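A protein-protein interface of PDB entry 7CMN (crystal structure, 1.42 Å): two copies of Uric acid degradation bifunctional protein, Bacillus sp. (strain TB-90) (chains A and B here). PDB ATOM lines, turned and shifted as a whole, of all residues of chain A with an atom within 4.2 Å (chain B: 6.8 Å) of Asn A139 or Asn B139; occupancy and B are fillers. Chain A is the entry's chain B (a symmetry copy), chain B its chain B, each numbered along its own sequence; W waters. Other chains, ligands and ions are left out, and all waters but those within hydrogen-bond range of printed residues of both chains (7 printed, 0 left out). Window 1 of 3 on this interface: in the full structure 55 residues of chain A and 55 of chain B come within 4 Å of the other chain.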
ATOM      1  N   LYS A 136     -22.170  -7.476  30.261  1.00  0.00           N
ATOM      2  CA  LYS A 136     -22.693  -6.151  30.548  1.00  0.00           C
ATOM      3  C   LYS A 136     -22.604  -5.301  29.289  1.00  0.00           C
ATOM      4  O   LYS A 136     -21.575  -5.298  28.599  1.00  0.00           O
ATOM      5  CB  LYS A 136     -21.917  -5.470  31.691  1.00  0.00           C
ATOM      6  CG  LYS A 136     -22.625  -4.226  32.255  1.00  0.00           C
ATOM      7  CD  LYS A 136     -21.770  -3.489  33.294  1.00  0.00           C
ATOM      8  CE  LYS A 136     -22.600  -2.541  34.174  1.00  0.00           C
ATOM      9  NZ  LYS A 136     -23.002  -3.201  35.505  1.00  0.00           N
ATOM     10  N   SER A 137     -23.714  -4.660  28.937  1.00  0.00           N
ATOM     11  CA  SER A 137     -23.775  -3.797  27.755  1.00  0.00           C
ATOM     12  C   SER A 137     -23.797  -2.323  28.122  1.00  0.00           C
ATOM     13  O   SER A 137     -24.607  -1.879  28.953  1.00  0.00           O
ATOM     14  CB  SER A 137     -24.991  -4.107  26.889  1.00  0.00           C
ATOM     15  OG  SER A 137     -24.995  -3.170  25.838  1.00  0.00           O
ATOM     16  N   ARG A 138     -22.927  -1.570  27.464  1.00  0.00           N
ATOM     17  CA  ARG A 138     -22.849  -0.125  27.614  1.00  0.00           C
ATOM     18  C   ARG A 138     -23.509   0.596  26.444  1.00  0.00           C
ATOM     19  O   ARG A 138     -23.236   1.781  26.194  1.00  0.00           O
ATOM     20  CB  ARG A 138     -21.394   0.314  27.828  1.00  0.00           C
ATOM     21  CG  ARG A 138     -20.845  -0.183  29.156  1.00  0.00           C
ATOM     22  CD  ARG A 138     -20.283  -1.560  29.069  1.00  0.00           C
ATOM     23  NE  ARG A 138     -18.979  -1.607  28.422  1.00  0.00           N
ATOM     24  CZ  ARG A 138     -18.342  -2.713  28.056  1.00  0.00           C
ATOM     25  NH1 ARG A 138     -18.905  -3.897  28.234  1.00  0.00           N
ATOM     26  NH2 ARG A 138     -17.136  -2.625  27.506  1.00  0.00           N
ATOM     27  N   ASN A 139     -24.390  -0.109  25.711  1.00  0.00           N
ATOM     28  CA  ASN A 139     -25.126   0.481  24.593  1.00  0.00           C
ATOM     29  C   ASN A 139     -26.476   0.946  25.102  1.00  0.00           C
ATOM     30  O   ASN A 139     -26.591   1.441  26.231  1.00  0.00           O
ATOM     31  CB  ASN A 139     -25.192  -0.511  23.464  1.00  0.00           C
ATOM     32  CG  ASN A 139     -23.795  -0.863  22.908  1.00  0.00           C
ATOM     33  OD1 ASN A 139     -22.871  -0.048  22.987  1.00  0.00           O
ATOM     34  ND2 ASN A 139     -23.612  -2.077  22.430  1.00  0.00           N
ATOM     35  N   GLU A 140     -27.501   0.875  24.264  1.00  0.00           N
ATOM     36  CA  GLU A 140     -28.788   1.453  24.582  1.00  0.00           C
ATOM     37  C   GLU A 140     -29.435   0.725  25.759  1.00  0.00           C
ATOM     38  O   GLU A 140     -29.149  -0.450  26.032  1.00  0.00           O
ATOM     39  CB  GLU A 140     -29.700   1.457  23.358  1.00  0.00           C
ATOM     40  CG  GLU A 140     -30.203   0.131  22.860  1.00  0.00           C
ATOM     41  CD  GLU A 140     -29.237  -0.594  21.956  1.00  0.00           C
ATOM     42  OE1 GLU A 140     -28.073  -0.148  21.793  1.00  0.00           O
ATOM     43  OE2 GLU A 140     -29.641  -1.642  21.397  1.00  0.00           O
ATOM     44  N   TYR A 141     -30.314   1.429  26.448  1.00  0.00           N
ATOM     45  CA  TYR A 141     -30.936   0.897  27.647  1.00  0.00           C
ATOM     46  C   TYR A 141     -32.331   1.486  27.801  1.00  0.00           C
ATOM     47  O   TYR A 141     -32.590   2.621  27.400  1.00  0.00           O
ATOM     48  CB  TYR A 141     -30.079   1.172  28.899  1.00  0.00           C
ATOM     49  CG  TYR A 141     -29.717   2.625  29.134  1.00  0.00           C
ATOM     50  CD1 TYR A 141     -28.609   3.208  28.504  1.00  0.00           C
ATOM     51  CD2 TYR A 141     -30.467   3.428  29.956  1.00  0.00           C
ATOM     52  CE1 TYR A 141     -28.290   4.549  28.696  1.00  0.00           C
ATOM     53  CE2 TYR A 141     -30.142   4.752  30.181  1.00  0.00           C
ATOM     54  CZ  TYR A 141     -29.064   5.308  29.508  1.00  0.00           C
ATOM     55  OH  TYR A 141     -28.748   6.613  29.725  1.00  0.00           O
ATOM     56  N   GLY A 167     -29.690   6.144  24.524  1.00  0.00           N
ATOM     57  CA  GLY A 167     -28.366   5.707  24.119  1.00  0.00           C
ATOM     58  C   GLY A 167     -28.323   4.875  22.859  1.00  0.00           C
ATOM     59  O   GLY A 167     -27.374   4.118  22.672  1.00  0.00           O
ATOM     60  N   PRO B 115     -16.491  -1.064  16.812  1.00  0.00           N
ATOM     61  CA  PRO B 115     -17.416  -2.106  16.350  1.00  0.00           C
ATOM     62  C   PRO B 115     -18.819  -1.593  16.138  1.00  0.00           C
ATOM     63  O   PRO B 115     -19.296  -0.690  16.820  1.00  0.00           O
ATOM     64  CB  PRO B 115     -17.386  -3.127  17.526  1.00  0.00           C
ATOM     65  CG  PRO B 115     -17.093  -2.297  18.713  1.00  0.00           C
ATOM     66  CD  PRO B 115     -16.189  -1.156  18.249  1.00  0.00           C
ATOM     67  N   GLU B 117     -22.837  -3.193  15.156  1.00  0.00           N
ATOM     68  CA  GLU B 117     -23.701  -4.360  15.214  1.00  0.00           C
ATOM     69  C   GLU B 117     -24.844  -4.215  14.244  1.00  0.00           C
ATOM     70  O   GLU B 117     -25.206  -3.126  13.809  1.00  0.00           O
ATOM     71  CB  GLU B 117     -24.221  -4.569  16.656  1.00  0.00           C
ATOM     72  CG  GLU B 117     -23.126  -4.945  17.572  1.00  0.00           C
ATOM     73  CD  GLU B 117     -23.505  -5.103  19.027  1.00  0.00           C
ATOM     74  OE1 GLU B 117     -24.700  -4.943  19.373  1.00  0.00           O
ATOM     75  OE2 GLU B 117     -22.579  -5.407  19.830  1.00  0.00           O
ATOM     76  N   LYS B 135     -25.488  -0.310  14.356  1.00  0.00           N
ATOM     77  CA  LYS B 135     -25.528   0.213  15.722  1.00  0.00           C
ATOM     78  C   LYS B 135     -24.115   0.280  16.277  1.00  0.00           C
ATOM     79  O   LYS B 135     -23.417  -0.739  16.332  1.00  0.00           O
ATOM     80  CB  LYS B 135     -26.446  -0.665  16.557  1.00  0.00           C
ATOM     81  CG  LYS B 135     -26.721  -0.162  17.950  1.00  0.00           C
ATOM     82  CD  LYS B 135     -27.575  -1.144  18.739  1.00  0.00           C
ATOM     83  CE  LYS B 135     -26.710  -2.183  19.457  1.00  0.00           C
ATOM     84  NZ  LYS B 135     -27.604  -3.088  20.228  1.00  0.00           N
ATOM     85  N   LYS B 136     -23.667   1.482  16.650  1.00  0.00           N
ATOM     86  CA  LYS B 136     -22.342   1.609  17.230  1.00  0.00           C
ATOM     87  C   LYS B 136     -22.333   0.937  18.596  1.00  0.00           C
ATOM     88  O   LYS B 136     -23.256   1.125  19.400  1.00  0.00           O
ATOM     89  CB  LYS B 136     -21.926   3.086  17.376  1.00  0.00           C
ATOM     90  CG  LYS B 136     -20.427   3.273  17.668  1.00  0.00           C
ATOM     91  CD  LYS B 136     -20.065   4.738  17.944  1.00  0.00           C
ATOM     92  CE  LYS B 136     -18.561   5.012  17.794  1.00  0.00           C
ATOM     93  NZ  LYS B 136     -18.216   5.567  16.400  1.00  0.00           N
ATOM     94  N   SER B 137     -21.344   0.076  18.816  1.00  0.00           N
ATOM     95  CA  SER B 137     -21.200  -0.638  20.087  1.00  0.00           C
ATOM     96  C   SER B 137     -20.061  -0.089  20.928  1.00  0.00           C
ATOM     97  O   SER B 137     -18.924   0.060  20.452  1.00  0.00           O
ATOM     98  CB  SER B 137     -20.982  -2.132  19.875  1.00  0.00           C
ATOM     99  OG  SER B 137     -20.773  -2.700  21.147  1.00  0.00           O
ATOM    100  N   ARG B 138     -20.372   0.169  22.190  1.00  0.00           N
ATOM    101  CA  ARG B 138     -19.402   0.622  23.174  1.00  0.00           C
ATOM    102  C   ARG B 138     -18.970  -0.510  24.098  1.00  0.00           C
ATOM    103  O   ARG B 138     -18.454  -0.268  25.201  1.00  0.00           O
ATOM    104  CB  ARG B 138     -19.946   1.833  23.946  1.00  0.00           C
ATOM    105  CG  ARG B 138     -20.096   3.052  23.049  1.00  0.00           C
ATOM    106  CD  ARG B 138     -21.402   3.082  22.332  1.00  0.00           C
ATOM    107  NE  ARG B 138     -22.515   3.474  23.185  1.00  0.00           N
ATOM    108  CZ  ARG B 138     -23.799   3.410  22.852  1.00  0.00           C
ATOM    109  NH1 ARG B 138     -24.159   2.923  21.676  1.00  0.00           N
ATOM    110  NH2 ARG B 138     -24.722   3.834  23.707  1.00  0.00           N
ATOM    111  N   ASN B 139     -19.171  -1.766  23.660  1.00  0.00           N
ATOM    112  CA  ASN B 139     -18.758  -2.939  24.430  1.00  0.00           C
ATOM    113  C   ASN B 139     -17.392  -3.377  23.938  1.00  0.00           C
ATOM    114  O   ASN B 139     -16.542  -2.540  23.603  1.00  0.00           O
ATOM    115  CB  ASN B 139     -19.824  -3.997  24.335  1.00  0.00           C
ATOM    116  CG  ASN B 139     -21.163  -3.539  24.954  1.00  0.00           C
ATOM    117  OD1 ASN B 139     -21.174  -2.702  25.862  1.00  0.00           O
ATOM    118  ND2 ASN B 139     -22.276  -4.008  24.426  1.00  0.00           N
ATOM    119  N   GLU B 140     -17.124  -4.674  23.958  1.00  0.00           N
ATOM    120  CA  GLU B 140     -15.799  -5.184  23.681  1.00  0.00           C
ATOM    121  C   GLU B 140     -15.406  -4.917  22.229  1.00  0.00           C
ATOM    122  O   GLU B 140     -16.259  -4.769  21.342  1.00  0.00           O
ATOM    123  CB  GLU B 140     -15.705  -6.669  24.020  1.00  0.00           C
ATOM    124  CG  GLU B 140     -16.467  -7.631  23.151  1.00  0.00           C
ATOM    125  CD  GLU B 140     -17.918  -7.786  23.529  1.00  0.00           C
ATOM    126  OE1 GLU B 140     -18.423  -7.039  24.405  1.00  0.00           O
ATOM    127  OE2 GLU B 140     -18.581  -8.670  22.935  1.00  0.00           O
ATOM    128  N   TYR B 141     -14.109  -4.862  21.993  1.00  0.00           N
ATOM    129  CA  TYR B 141     -13.592  -4.522  20.679  1.00  0.00           C
ATOM    130  C   TYR B 141     -12.257  -5.218  20.461  1.00  0.00           C
ATOM    131  O   TYR B 141     -11.498  -5.448  21.402  1.00  0.00           O
ATOM    132  CB  TYR B 141     -13.455  -2.996  20.502  1.00  0.00           C
ATOM    133  CG  TYR B 141     -12.625  -2.291  21.557  1.00  0.00           C
ATOM    134  CD1 TYR B 141     -13.188  -1.889  22.775  1.00  0.00           C
ATOM    135  CD2 TYR B 141     -11.290  -2.036  21.367  1.00  0.00           C
ATOM    136  CE1 TYR B 141     -12.422  -1.266  23.756  1.00  0.00           C
ATOM    137  CE2 TYR B 141     -10.525  -1.389  22.320  1.00  0.00           C
ATOM    138  CZ  TYR B 141     -11.106  -1.043  23.531  1.00  0.00           C
ATOM    139  OH  TYR B 141     -10.352  -0.411  24.471  1.00  0.00           O
ATOM    140  N   ALA B 166     -10.456  -6.293  23.904  1.00  0.00           N
ATOM    141  CA  ALA B 166     -10.485  -5.431  25.060  1.00  0.00           C
ATOM    142  C   ALA B 166     -11.924  -5.129  25.448  1.00  0.00           C
ATOM    143  O   ALA B 166     -12.838  -5.215  24.638  1.00  0.00           O
ATOM    144  CB  ALA B 166      -9.783  -4.100  24.733  1.00  0.00           C
ATOM    145  N   GLY B 167     -12.133  -4.871  26.727  1.00  0.00           N
ATOM    146  CA  GLY B 167     -13.422  -4.371  27.170  1.00  0.00           C
ATOM    147  C   GLY B 167     -14.503  -5.417  27.308  1.00  0.00           C
ATOM    148  O   GLY B 167     -15.680  -5.075  27.247  1.00  0.00           O
ATOM    149  N   LEU B 168     -14.128  -6.684  27.528  1.00  0.00           N
ATOM    150  CA  LEU B 168     -15.111  -7.746  27.704  1.00  0.00           C
ATOM    151  C   LEU B 168     -15.525  -7.774  29.171  1.00  0.00           C
ATOM    152  O   LEU B 168     -14.673  -7.906  30.054  1.00  0.00           O
ATOM    153  CB  LEU B 168     -14.558  -9.056  27.217  1.00  0.00           C
ATOM    154  CG  LEU B 168     -15.538 -10.248  27.256  1.00  0.00           C
ATOM    155  CD1 LEU B 168     -16.708 -10.028  26.342  1.00  0.00           C
ATOM    156  CD2 LEU B 168     -14.825 -11.531  26.939  1.00  0.00           C
ATOM    157  N   GLN B 169     -16.813  -7.583  29.441  1.00  0.00           N
ATOM    158  CA  GLN B 169     -17.317  -7.486  30.812  1.00  0.00           C
ATOM    159  C   GLN B 169     -18.327  -8.594  31.013  1.00  0.00           C
ATOM    160  O   GLN B 169     -19.399  -8.570  30.416  1.00  0.00           O
ATOM    161  CB  GLN B 169     -17.942  -6.105  31.024  1.00  0.00           C
ATOM    162  CG  GLN B 169     -16.978  -4.932  30.802  1.00  0.00           C
ATOM    163  CD  GLN B 169     -17.549  -3.583  31.256  1.00  0.00           C
ATOM    164  OE1 GLN B 169     -18.642  -3.493  31.764  1.00  0.00           O
ATOM    165  NE2 GLN B 169     -16.761  -2.545  31.076  1.00  0.00           N
HETATM  166  O   HOH W   1     -25.543  -4.196  21.929  1.00  0.00           O
HETATM  167  O   HOH W   2     -25.396   4.059  26.778  1.00  0.00           O
HETATM  168  O   HOH W   3     -17.934   1.152  27.359  1.00  0.00           O
HETATM  169  O   HOH W   4     -18.536  -6.601  27.212  1.00  0.00           O
HETATM  170  O   HOH W   5     -26.596   1.883  20.462  1.00  0.00           O
HETATM  171  O   HOH W   6     -15.341  -0.821  25.648  1.00  0.00           O
HETATM  172  O   HOH W   7     -21.764   3.966  26.190  1.00  0.00           O
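The side-chain hydroxyl of Ser B137 lies within hydrogen-bond range of the side-chain amide nitrogen of Asn A139 (3.2 Å).
OD1 of Asn B139 is in hydrogen-bond range of N of Arg A138 (2.6 Å).
The backbone carbonyl oxygen of Gly B167 is in hydrogen-bond range of the guanidinium group of Arg A138 (2.9 Å).
The guanidinium group of Arg B138 lies within hydrogen-bond range of the backbone carbonyl oxygen of Gly A167 (2.9 Å).
NZ of Lys B135 lies within salt-bridge range of OE2 of Glu A140 (2.8 Å).
N of Arg B138 sits at hydrogen-bond distance from OD1 of Asn A139 (2.6 Å).
ND2 of Asn A139 lies close to ND2 of Asn B139 (3.1 Å).
OG of Ser A137 lies within hydrogen-bond range of ND2 of Asn B139 (3.2 Å).
O of Gln B169 sits at hydrogen-bond distance from N of Lys A136, at 3.0 Å.
O of Lys A136 is in hydrogen-bond range of NH1 of Arg A138 (3.0 Å).
The backbone carbonyl oxygen (O) of Lys B136 sits at hydrogen-bond distance from the guanidinium group (NH1) of Arg B138 (3.0 Å).
The backbone carbonyl oxygen of Pro B115 is in hydrogen-bond range of the backbone NH of Ser B137 (3.0 Å).
OG of Ser A137 lies within hydrogen-bond range of N of Asn A139, 3.1 Å away.
The side-chain amino group (NZ) of Lys B135 lies within salt-bridge range of the side-chain carboxylate (OE1) of Glu B117, 3.6 Å away.
OG of Ser B137 sits at hydrogen-bond distance from N of Asn B139 (3.1 Å).
Lys A136 touches Asn B139 (O to OD1, 3.8 Å).
O of Arg A138 touches NE of Arg B138, 3.5 Å away.
NH1 of Arg A138 touches CD of Gln B169, 3.3 Å away.
O of Lys B136 touches OD1 of Asn A139 (3.8 Å).
Of the printed residues of chain B, Gly A167 touches Arg B138.
Of the printed residues of chain A, Arg B138 touches Arg A138 (3.5 Å), Asn A139 (2.6 Å) and Gly A167 (2.9 Å).
Of the printed residues of chain A, Asn B139 touches Lys A136 (3.8 Å), Ser A137 (3.2 Å), Arg A138 (2.6 Å) and Asn A139 (3.1 Å).
Of the printed residues of chain A, Gly B167 touches Arg A138.
The nearest printed residue of chain A that does not touch Asn B139 is Glu A140 (7.2 Å).
Of the 13 printed residues of chain B, 7 touch a printed residue of chain A.
Printed residues of chain B that touch a printed residue of chain A: Lys B135, Lys B136, Ser B137, Arg B138, Asn B139, Gly B167 and Gln B169.
Of the 7 printed residues of chain A, 6 touch a printed residue of chain B.
Printed residues of chain A that touch a printed residue of chain B: Lys A136, Ser A137, Arg A138, Asn A139, Glu A140 and Gly A167.
Among the printed residues, 13 pairs touch across the chains.
Among the printed residues, Asp or Glu carboxylates within 4 Å of a Lys or Arg side-chain nitrogen of the other chain: Glu A140 with Lys B135.
Ser A137 touches Asn B139, and with the chains exchanged Asn A139 touches Ser B137.
Arg A138 touches Asn B139, and with the chains exchanged Asn A139 touches Arg B138.
Arg A138 touches Gly B167, and with the chains exchanged Gly A167 touches Arg B138.
Asn B139 touches its own counterpart, Asn A139.
Positions printed for both chains: 136, 137, 138, 139, 140, 141 and 167.
Water W7 bridges O of Arg A138 (2.6 Å) and NE of Arg B138 (3.1 Å).
Water W3 lies within hydrogen-bond range of O of Arg B138 (2.6 Å) and NE of Arg A138 (3.1 Å).
Water W1 lies within hydrogen-bond range of the side-chain carboxylate of Glu B117 (2.8 Å), the side-chain amino group of Lys B135 (2.9 Å) and the side-chain amide nitrogen of Asn A139 (2.9 Å).
Water W4 lies within hydrogen-bond range of OE1 of Glu B140 (2.8 Å), NH1 of Arg A138 (2.9 Å), N of Gln B169 (3.0 Å) and O of Gly B167 (3.2 Å).
Water W2 lies within hydrogen-bond range of the backbone carbonyl oxygen (O) of Asn A139, the guanidinium group (NH2) of Arg B138 and the backbone carbonyl oxygen (O) of Arg A138.
Water W6 lies within hydrogen-bond range of the backbone carbonyl oxygen of Asn B139 (2.9 Å), the guanidinium group of Arg A138 (3.2 Å) and the backbone carbonyl oxygen of Arg B138 (3.2 Å).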
